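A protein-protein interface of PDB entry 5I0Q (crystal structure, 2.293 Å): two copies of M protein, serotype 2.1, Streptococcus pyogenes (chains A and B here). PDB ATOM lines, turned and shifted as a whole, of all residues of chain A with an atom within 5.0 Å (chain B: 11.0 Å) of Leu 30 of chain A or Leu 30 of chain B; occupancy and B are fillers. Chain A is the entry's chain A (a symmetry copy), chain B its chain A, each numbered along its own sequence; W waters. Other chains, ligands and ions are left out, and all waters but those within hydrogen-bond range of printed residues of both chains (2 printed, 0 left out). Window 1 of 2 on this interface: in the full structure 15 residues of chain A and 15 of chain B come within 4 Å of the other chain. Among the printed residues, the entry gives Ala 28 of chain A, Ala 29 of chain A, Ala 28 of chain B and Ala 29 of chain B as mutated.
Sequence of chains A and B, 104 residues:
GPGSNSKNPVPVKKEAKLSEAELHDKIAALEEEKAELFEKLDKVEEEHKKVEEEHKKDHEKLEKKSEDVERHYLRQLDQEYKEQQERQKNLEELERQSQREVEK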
ATOM      1  N   LYS A  26     -12.179  -1.045 -27.662  1.00  0.00           N
ATOM      2  CA  LYS A  26     -10.943  -0.795 -28.390  1.00  0.00           C
ATOM      3  C   LYS A  26      -9.921  -0.043 -27.526  1.00  0.00           C
ATOM      4  O   LYS A  26      -8.736  -0.360 -27.533  1.00  0.00           O
ATOM      5  CB  LYS A  26     -11.225  -0.010 -29.669  1.00  0.00           C
ATOM      6  CG  LYS A  26      -9.980   0.278 -30.512  1.00  0.00           C
ATOM      7  CD  LYS A  26      -9.324  -0.995 -31.094  1.00  0.00           C
ATOM      8  CE  LYS A  26      -8.106  -0.621 -31.943  1.00  0.00           C
ATOM      9  NZ  LYS A  26      -7.429  -1.786 -32.609  1.00  0.00           N
ATOM     10  N   ILE A  27     -10.384   0.959 -26.787  1.00  0.00           N
ATOM     11  CA  ILE A  27      -9.521   1.672 -25.863  1.00  0.00           C
ATOM     12  C   ILE A  27      -8.914   0.717 -24.814  1.00  0.00           C
ATOM     13  O   ILE A  27      -7.712   0.751 -24.560  1.00  0.00           O
ATOM     14  CB  ILE A  27     -10.292   2.805 -25.187  1.00  0.00           C
ATOM     15  CG1 ILE A  27     -10.568   3.910 -26.229  1.00  0.00           C
ATOM     16  CG2 ILE A  27      -9.539   3.314 -23.965  1.00  0.00           C
ATOM     17  CD1 ILE A  27     -11.504   5.049 -25.754  1.00  0.00           C
ATOM     18  N   ALA A  28      -9.734  -0.161 -24.257  1.00  0.00           N
ATOM     19  CA  ALA A  28      -9.265  -1.155 -23.298  1.00  0.00           C
ATOM     20  C   ALA A  28      -8.186  -2.055 -23.895  1.00  0.00           C
ATOM     21  O   ALA A  28      -7.136  -2.240 -23.294  1.00  0.00           O
ATOM     22  CB  ALA A  28     -10.427  -2.006 -22.803  1.00  0.00           C
ATOM     23  N   ALA A  29      -8.459  -2.614 -25.074  1.00  0.00           N
ATOM     24  CA  ALA A  29      -7.504  -3.490 -25.742  1.00  0.00           C
ATOM     25  C   ALA A  29      -6.202  -2.752 -25.999  1.00  0.00           C
ATOM     26  O   ALA A  29      -5.130  -3.313 -25.807  1.00  0.00           O
ATOM     27  CB  ALA A  29      -8.076  -4.025 -27.060  1.00  0.00           C
ATOM     28  N   LEU A  30      -6.286  -1.492 -26.418  1.00  0.00           N
ATOM     29  CA  LEU A  30      -5.078  -0.748 -26.747  1.00  0.00           C
ATOM     30  C   LEU A  30      -4.253  -0.545 -25.489  1.00  0.00           C
ATOM     31  O   LEU A  30      -3.041  -0.693 -25.535  1.00  0.00           O
ATOM     32  CB  LEU A  30      -5.402   0.592 -27.412  1.00  0.00           C
ATOM     33  CG  LEU A  30      -5.719   0.553 -28.920  1.00  0.00           C
ATOM     34  CD1 LEU A  30      -6.323   1.861 -29.373  1.00  0.00           C
ATOM     35  CD2 LEU A  30      -4.488   0.249 -29.752  1.00  0.00           C
ATOM     36  N   GLU A  31      -4.906  -0.235 -24.366  1.00  0.00           N
ATOM     37  CA  GLU A  31      -4.210  -0.067 -23.099  1.00  0.00           C
ATOM     38  C   GLU A  31      -3.573  -1.376 -22.608  1.00  0.00           C
ATOM     39  O   GLU A  31      -2.463  -1.342 -22.065  1.00  0.00           O
ATOM     40  CB  GLU A  31      -5.159   0.501 -22.016  1.00  0.00           C
ATOM     41  CG  GLU A  31      -5.531   1.958 -22.257  1.00  0.00           C
ATOM     42  CD  GLU A  31      -6.534   2.523 -21.261  1.00  0.00           C
ATOM     43  OE1 GLU A  31      -7.164   1.773 -20.481  1.00  0.00           O
ATOM     44  OE2 GLU A  31      -6.666   3.765 -21.233  1.00  0.00           O
ATOM     45  N   GLU A  32      -4.249  -2.519 -22.771  1.00  0.00           N
ATOM     46  CA  GLU A  32      -3.622  -3.780 -22.333  1.00  0.00           C
ATOM     47  C   GLU A  32      -2.458  -4.128 -23.237  1.00  0.00           C
ATOM     48  O   GLU A  32      -1.493  -4.730 -22.784  1.00  0.00           O
ATOM     49  CB  GLU A  32      -4.564  -4.990 -22.312  1.00  0.00           C
ATOM     50  CG  GLU A  32      -6.014  -4.731 -22.416  1.00  0.00           C
ATOM     51  CD  GLU A  32      -6.743  -5.045 -21.159  1.00  0.00           C
ATOM     52  OE1 GLU A  32      -6.054  -5.278 -20.145  1.00  0.00           O
ATOM     53  OE2 GLU A  32      -7.998  -5.054 -21.183  1.00  0.00           O
ATOM     54  N   GLU A  33      -2.549  -3.753 -24.511  1.00  0.00           N
ATOM     55  CA  GLU A  33      -1.459  -4.020 -25.440  1.00  0.00           C
ATOM     56  C   GLU A  33      -0.251  -3.144 -25.143  1.00  0.00           C
ATOM     57  O   GLU A  33       0.868  -3.612 -25.270  1.00  0.00           O
ATOM     58  CB  GLU A  33      -1.904  -3.824 -26.893  1.00  0.00           C
ATOM     59  CG  GLU A  33      -2.920  -4.845 -27.363  1.00  0.00           C
ATOM     60  CD  GLU A  33      -3.687  -4.389 -28.607  1.00  0.00           C
ATOM     61  OE1 GLU A  33      -3.250  -3.433 -29.288  1.00  0.00           O
ATOM     62  OE2 GLU A  33      -4.733  -5.001 -28.903  1.00  0.00           O
ATOM     63  N   LYS A  34      -0.466  -1.881 -24.768  1.00  0.00           N
ATOM     64  CA  LYS A  34       0.639  -1.062 -24.284  1.00  0.00           C
ATOM     65  C   LYS A  34       1.303  -1.723 -23.075  1.00  0.00           C
ATOM     66  O   LYS A  34       2.520  -1.818 -23.025  1.00  0.00           O
ATOM     67  CB  LYS A  34       0.189   0.354 -23.910  1.00  0.00           C
ATOM     68  CG  LYS A  34       0.326   1.329 -25.042  1.00  0.00           C
ATOM     69  CD  LYS A  34      -0.141   2.733 -24.693  1.00  0.00           C
ATOM     70  CE  LYS A  34       0.835   3.435 -23.783  1.00  0.00           C
ATOM     71  NZ  LYS A  34       0.353   4.820 -23.493  1.00  0.00           N
ATOM     72  N   GLU B  22     -15.252  10.822 -28.220  1.00  0.00           N
ATOM     73  CA  GLU B  22     -13.840  11.232 -28.374  1.00  0.00           C
ATOM     74  C   GLU B  22     -13.009  10.227 -27.694  1.00  0.00           C
ATOM     75  O   GLU B  22     -11.868  10.402 -27.247  1.00  0.00           O
ATOM     76  CB  GLU B  22     -13.626  12.621 -27.889  1.00  0.00           C
ATOM     77  CG  GLU B  22     -14.127  13.519 -28.980  1.00  0.00           C
ATOM     78  CD  GLU B  22     -14.473  12.708 -30.209  1.00  0.00           C
ATOM     79  OE1 GLU B  22     -13.513  12.236 -30.867  1.00  0.00           O
ATOM     80  OE2 GLU B  22     -15.693  12.496 -30.470  1.00  0.00           O
ATOM     81  N   LEU B  23     -13.741   9.155 -27.618  1.00  0.00           N
ATOM     82  CA  LEU B  23     -13.309   7.843 -27.811  1.00  0.00           C
ATOM     83  C   LEU B  23     -12.382   7.808 -29.008  1.00  0.00           C
ATOM     84  O   LEU B  23     -11.338   7.171 -28.935  1.00  0.00           O
ATOM     85  CB  LEU B  23     -14.561   7.013 -27.997  1.00  0.00           C
ATOM     86  CG  LEU B  23     -15.399   7.393 -26.759  1.00  0.00           C
ATOM     87  CD1 LEU B  23     -16.861   6.882 -26.765  1.00  0.00           C
ATOM     88  CD2 LEU B  23     -14.664   6.876 -25.551  1.00  0.00           C
ATOM     89  N   HIS B  24     -12.742   8.506 -30.094  1.00  0.00           N
ATOM     90  CA  HIS B  24     -11.968   8.398 -31.318  1.00  0.00           C
ATOM     91  C   HIS B  24     -10.585   9.019 -31.125  1.00  0.00           C
ATOM     92  O   HIS B  24      -9.593   8.407 -31.534  1.00  0.00           O
ATOM     93  CB  HIS B  24     -12.685   9.048 -32.507  1.00  0.00           C
ATOM     94  CG  HIS B  24     -13.713   8.161 -33.142  1.00  0.00           C
ATOM     95  ND1 HIS B  24     -13.413   7.306 -34.172  1.00  0.00           N
ATOM     96  CD2 HIS B  24     -15.028   7.977 -32.861  1.00  0.00           C
ATOM     97  CE1 HIS B  24     -14.503   6.637 -34.521  1.00  0.00           C
ATOM     98  NE2 HIS B  24     -15.494   7.029 -33.740  1.00  0.00           N
ATOM     99  N   ASP B  25     -10.506  10.200 -30.499  1.00  0.00           N
ATOM    100  CA  ASP B  25      -9.207  10.851 -30.293  1.00  0.00           C
ATOM    101  C   ASP B  25      -8.329  10.023 -29.356  1.00  0.00           C
ATOM    102  O   ASP B  25      -7.118   9.926 -29.546  1.00  0.00           O
ATOM    103  CB  ASP B  25      -9.365  12.265 -29.714  1.00  0.00           C
ATOM    104  CG  ASP B  25      -9.812  13.281 -30.747  1.00  0.00           C
ATOM    105  OD1 ASP B  25      -9.912  12.935 -31.949  1.00  0.00           O
ATOM    106  OD2 ASP B  25     -10.048  14.442 -30.356  1.00  0.00           O
ATOM    107  N   LYS B  26      -8.954   9.431 -28.345  1.00  0.00           N
ATOM    108  CA  LYS B  26      -8.244   8.597 -27.383  1.00  0.00           C
ATOM    109  C   LYS B  26      -7.638   7.357 -28.052  1.00  0.00           C
ATOM    110  O   LYS B  26      -6.506   6.978 -27.766  1.00  0.00           O
ATOM    111  CB  LYS B  26      -9.179   8.176 -26.250  1.00  0.00           C
ATOM    112  CG  LYS B  26      -8.509   7.314 -25.177  1.00  0.00           C
ATOM    113  CD  LYS B  26      -7.410   8.061 -24.385  1.00  0.00           C
ATOM    114  CE  LYS B  26      -6.810   7.141 -23.319  1.00  0.00           C
ATOM    115  NZ  LYS B  26      -5.773   7.791 -22.447  1.00  0.00           N
ATOM    116  N   ILE B  27      -8.398   6.721 -28.937  1.00  0.00           N
ATOM    117  CA  ILE B  27      -7.884   5.595 -29.697  1.00  0.00           C
ATOM    118  C   ILE B  27      -6.645   5.996 -30.525  1.00  0.00           C
ATOM    119  O   ILE B  27      -5.634   5.298 -30.512  1.00  0.00           O
ATOM    120  CB  ILE B  27      -8.978   5.021 -30.596  1.00  0.00           C
ATOM    121  CG1 ILE B  27     -10.029   4.314 -29.712  1.00  0.00           C
ATOM    122  CG2 ILE B  27      -8.378   4.106 -31.656  1.00  0.00           C
ATOM    123  CD1 ILE B  27     -11.303   3.840 -30.454  1.00  0.00           C
ATOM    124  N   ALA B  28      -6.711   7.141 -31.189  1.00  0.00           N
ATOM    125  CA  ALA B  28      -5.584   7.654 -31.956  1.00  0.00           C
ATOM    126  C   ALA B  28      -4.349   7.860 -31.081  1.00  0.00           C
ATOM    127  O   ALA B  28      -3.266   7.405 -31.426  1.00  0.00           O
ATOM    128  CB  ALA B  28      -5.956   8.967 -32.634  1.00  0.00           C
ATOM    129  N   ALA B  29      -4.523   8.553 -29.955  1.00  0.00           N
ATOM    130  CA  ALA B  29      -3.417   8.810 -29.040  1.00  0.00           C
ATOM    131  C   ALA B  29      -2.817   7.501 -28.556  1.00  0.00           C
ATOM    132  O   ALA B  29      -1.603   7.377 -28.473  1.00  0.00           O
ATOM    133  CB  ALA B  29      -3.877   9.655 -27.846  1.00  0.00           C
ATOM    134  N   LEU B  30      -3.662   6.520 -28.247  1.00  0.00           N
ATOM    135  CA  LEU B  30      -3.158   5.263 -27.713  1.00  0.00           C
ATOM    136  C   LEU B  30      -2.326   4.563 -28.773  1.00  0.00           C
ATOM    137  O   LEU B  30      -1.273   4.032 -28.455  1.00  0.00           O
ATOM    138  CB  LEU B  30      -4.293   4.360 -27.223  1.00  0.00           C
ATOM    139  CG  LEU B  30      -4.858   4.665 -25.821  1.00  0.00           C
ATOM    140  CD1 LEU B  30      -6.156   3.928 -25.596  1.00  0.00           C
ATOM    141  CD2 LEU B  30      -3.874   4.305 -24.725  1.00  0.00           C
ATOM    142  N   GLU B  31      -2.781   4.586 -30.028  1.00  0.00           N
ATOM    143  CA  GLU B  31      -2.032   3.983 -31.122  1.00  0.00           C
ATOM    144  C   GLU B  31      -0.698   4.701 -31.377  1.00  0.00           C
ATOM    145  O   GLU B  31       0.301   4.034 -31.667  1.00  0.00           O
ATOM    146  CB  GLU B  31      -2.876   3.953 -32.419  1.00  0.00           C
ATOM    147  CG  GLU B  31      -4.022   2.953 -32.362  1.00  0.00           C
ATOM    148  CD  GLU B  31      -4.926   2.959 -33.585  1.00  0.00           C
ATOM    149  OE1 GLU B  31      -4.859   3.879 -34.432  1.00  0.00           O
ATOM    150  OE2 GLU B  31      -5.702   1.990 -33.723  1.00  0.00           O
ATOM    151  N   GLU B  32      -0.660   6.036 -31.290  1.00  0.00           N
ATOM    152  CA  GLU B  32       0.628   6.721 -31.499  1.00  0.00           C
ATOM    153  C   GLU B  32       1.565   6.438 -30.343  1.00  0.00           C
ATOM    154  O   GLU B  32       2.773   6.390 -30.536  1.00  0.00           O
ATOM    155  CB  GLU B  32       0.527   8.245 -31.645  1.00  0.00           C
ATOM    156  CG  GLU B  32      -0.813   8.823 -31.876  1.00  0.00           C
ATOM    157  CD  GLU B  32      -0.960   9.399 -33.237  1.00  0.00           C
ATOM    158  OE1 GLU B  32      -0.054   9.154 -34.060  1.00  0.00           O
ATOM    159  OE2 GLU B  32      -1.978  10.091 -33.486  1.00  0.00           O
ATOM    160  N   GLU B  33       1.012   6.259 -29.147  1.00  0.00           N
ATOM    161  CA  GLU B  33       1.838   5.950 -27.987  1.00  0.00           C
ATOM    162  C   GLU B  33       2.406   4.540 -28.071  1.00  0.00           C
ATOM    163  O   GLU B  33       3.541   4.332 -27.674  1.00  0.00           O
ATOM    164  CB  GLU B  33       1.055   6.122 -26.681  1.00  0.00           C
ATOM    165  CG  GLU B  33       0.685   7.559 -26.377  1.00  0.00           C
ATOM    166  CD  GLU B  33      -0.456   7.676 -25.362  1.00  0.00           C
ATOM    167  OE1 GLU B  33      -0.769   6.683 -24.667  1.00  0.00           O
ATOM    168  OE2 GLU B  33      -1.036   8.775 -25.262  1.00  0.00           O
ATOM    169  N   LYS B  34       1.627   3.576 -28.565  1.00  0.00           N
ATOM    170  CA  LYS B  34       2.183   2.258 -28.850  1.00  0.00           C
ATOM    171  C   LYS B  34       3.343   2.371 -29.841  1.00  0.00           C
ATOM    172  O   LYS B  34       4.392   1.787 -29.619  1.00  0.00           O
ATOM    173  CB  LYS B  34       1.130   1.293 -29.406  1.00  0.00           C
ATOM    174  CG  LYS B  34       0.465   0.477 -28.335  1.00  0.00           C
ATOM    175  CD  LYS B  34      -0.600  -0.467 -28.868  1.00  0.00           C
ATOM    176  CE  LYS B  34       0.007  -1.645 -29.588  1.00  0.00           C
ATOM    177  NZ  LYS B  34      -1.074  -2.560 -30.066  1.00  0.00           N
ATOM    178  N   ALA B  35       3.148   3.119 -30.926  1.00  0.00           N
ATOM    179  CA  ALA B  35       4.187   3.266 -31.950  1.00  0.00           C
ATOM    180  C   ALA B  35       5.476   3.812 -31.343  1.00  0.00           C
ATOM    181  O   ALA B  35       6.563   3.392 -31.716  1.00  0.00           O
ATOM    182  CB  ALA B  35       3.714   4.169 -33.077  1.00  0.00           C
ATOM    183  N   GLU B  36       5.332   4.745 -30.403  1.00  0.00           N
ATOM    184  CA  GLU B  36       6.460   5.331 -29.678  1.00  0.00           C
ATOM    185  C   GLU B  36       7.181   4.283 -28.819  1.00  0.00           C
ATOM    186  O   GLU B  36       8.410   4.243 -28.762  1.00  0.00           O
ATOM    187  CB  GLU B  36       5.969   6.484 -28.796  1.00  0.00           C
ATOM    188  CG  GLU B  36       7.006   7.533 -28.467  1.00  0.00           C
ATOM    189  CD  GLU B  36       7.207   8.515 -29.604  1.00  0.00           C
ATOM    190  OE1 GLU B  36       6.359   8.531 -30.524  1.00  0.00           O
ATOM    191  OE2 GLU B  36       8.211   9.264 -29.581  1.00  0.00           O
ATOM    192  N   LEU B  37       6.402   3.447 -28.140  1.00  0.00           N
ATOM    193  CA  LEU B  37       6.935   2.287 -27.432  1.00  0.00           C
ATOM    194  C   LEU B  37       7.722   1.350 -28.355  1.00  0.00           C
ATOM    195  O   LEU B  37       8.778   0.848 -27.986  1.00  0.00           O
ATOM    196  CB  LEU B  37       5.804   1.508 -26.771  1.00  0.00           C
ATOM    197  CG  LEU B  37       5.566   1.742 -25.291  1.00  0.00           C
ATOM    198  CD1 LEU B  37       6.860   1.487 -24.541  1.00  0.00           C
ATOM    199  CD2 LEU B  37       5.062   3.162 -25.072  1.00  0.00           C
ATOM    200  N   PHE B  38       7.192   1.095 -29.544  1.00  0.00           N
ATOM    201  CA  PHE B  38       7.872   0.228 -30.503  1.00  0.00           C
ATOM    202  C   PHE B  38       9.215   0.824 -30.913  1.00  0.00           C
ATOM    203  O   PHE B  38      10.202   0.101 -31.017  1.00  0.00           O
ATOM    204  CB  PHE B  38       7.003  -0.015 -31.736  1.00  0.00           C
ATOM    205  CG  PHE B  38       5.900  -1.026 -31.526  1.00  0.00           C
ATOM    206  CD1 PHE B  38       6.183  -2.303 -31.074  1.00  0.00           C
ATOM    207  CD2 PHE B  38       4.579  -0.706 -31.816  1.00  0.00           C
ATOM    208  CE1 PHE B  38       5.172  -3.234 -30.909  1.00  0.00           C
ATOM    209  CE2 PHE B  38       3.562  -1.641 -31.639  1.00  0.00           C
ATOM    210  CZ  PHE B  38       3.866  -2.904 -31.190  1.00  0.00           C
HETATM  211  O   HOH W   1      -5.243  -0.615 -33.800  1.00  0.00           O
HETATM  212  O   HOH W   2      -4.895   5.701 -20.889  1.00  0.00           O
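Among the printed residues, merely in contact across the chains: Lys 34 of chain A with Lys 34 of chain B, Ile 27 of chain A with Ile 27 of chain B, Ile 27 of chain A with Leu 23 of chain B, Leu 30 of chain A with Ile 27 of chain B, Ile 27 of chain A with Leu 30 of chain B, Leu 30 of chain A with Glu 31 of chain B, Glu 31 of chain A with Leu 30 of chain B, Ile 27 of chain A with Lys 26 of chain B, Lys 26 of chain A with Ile 27 of chain B, Leu 30 of chain A with Leu 30 of chain B, Lys 26 of chain A with Glu 31 of chain B and Glu 31 of chain A with Lys 26 of chain B.
Printed residues of chain B within 4 Å of Lys 26 of chain A: Ile 27 and Glu 31.
Ala 28 of chain A touches none of the printed residues of chain B.
No residue of chain B comes within 4 Å of Ala 29 of chain A.
Leu 30 of chain A touches three residues of chain B.
Glu 31 of chain A touches just these residues of chain B: Lys 26 (3.97 Å) and Leu 30 (3.8 Å).
Lys 34 of chain A touches two residues of chain B.
Glu 22 of chain B touches none of the printed residues of chain A.
Of the printed residues of chain A, Leu 23 of chain B touches Ile 27 (3.7 Å).
Of the printed residues of chain A, Lys 26 of chain B touches Ile 27 (3.8 Å) and Glu 31 (3.97 Å).
Leu 30 of chain B touches just these residues of chain A: Ile 27 (3.7 Å), Leu 30 (3.9 Å) and Glu 31 (3.8 Å).
Printed residues of chain A within 4 Å of Glu 31 of chain B: Lys 26 (3.97 Å) and Leu 30 (3.8 Å).
The nearest residue of chain A that does not touch Leu 30 of chain B is Lys 34 of chain A (4.1 Å).
Printed residues of chain A that touch a printed residue of chain B: Lys 26, Ile 27, Leu 30, Glu 31, Glu 33 and Lys 34.
Printed residues of chain B that touch a printed residue of chain A: Leu 23, Lys 26, Ile 27, Leu 30, Glu 31, Glu 33 and Lys 34.
Among the printed residues, 14 pairs touch across the chains.
Among the printed residues, Asp or Glu carboxylates within 4 Å of a Lys or Arg side-chain nitrogen of the other chain: Glu 33 of chain A with Lys 34 of chain B (2.5 Å) and Lys 34 of chain A with Glu 33 of chain B (2.5 Å).
NZ of Lys 34 of chain B lies within salt-bridge range of OE1 of Glu 33 of chain A.
NZ of Lys 34 of chain A is in salt-bridge range of OE1 of Glu 33 of chain B (2.5 Å).
Water W2 bridges the side-chain carboxylate (OE2) of Glu 31 of chain A and the side-chain amino group (NZ) of Lys 26 of chain B.
Water W1 bridges OE2 of Glu 31 of chain B (2.6 Å) and NZ of Lys 26 of chain A (2.8 Å).
Ile 27 of chain A touches Leu 30 of chain B, and with the chains exchanged Leu 30 of chain A touches Ile 27 of chain B.
Leu 30 of chain B touches its own counterpart, Leu 30 of chain A.
Leu 30 of chain A touches Glu 31 of chain B, and with the chains exchanged Glu 31 of chain A touches Leu 30 of chain B.
Lys 34 of chain B touches its own counterpart, Lys 34 of chain A.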
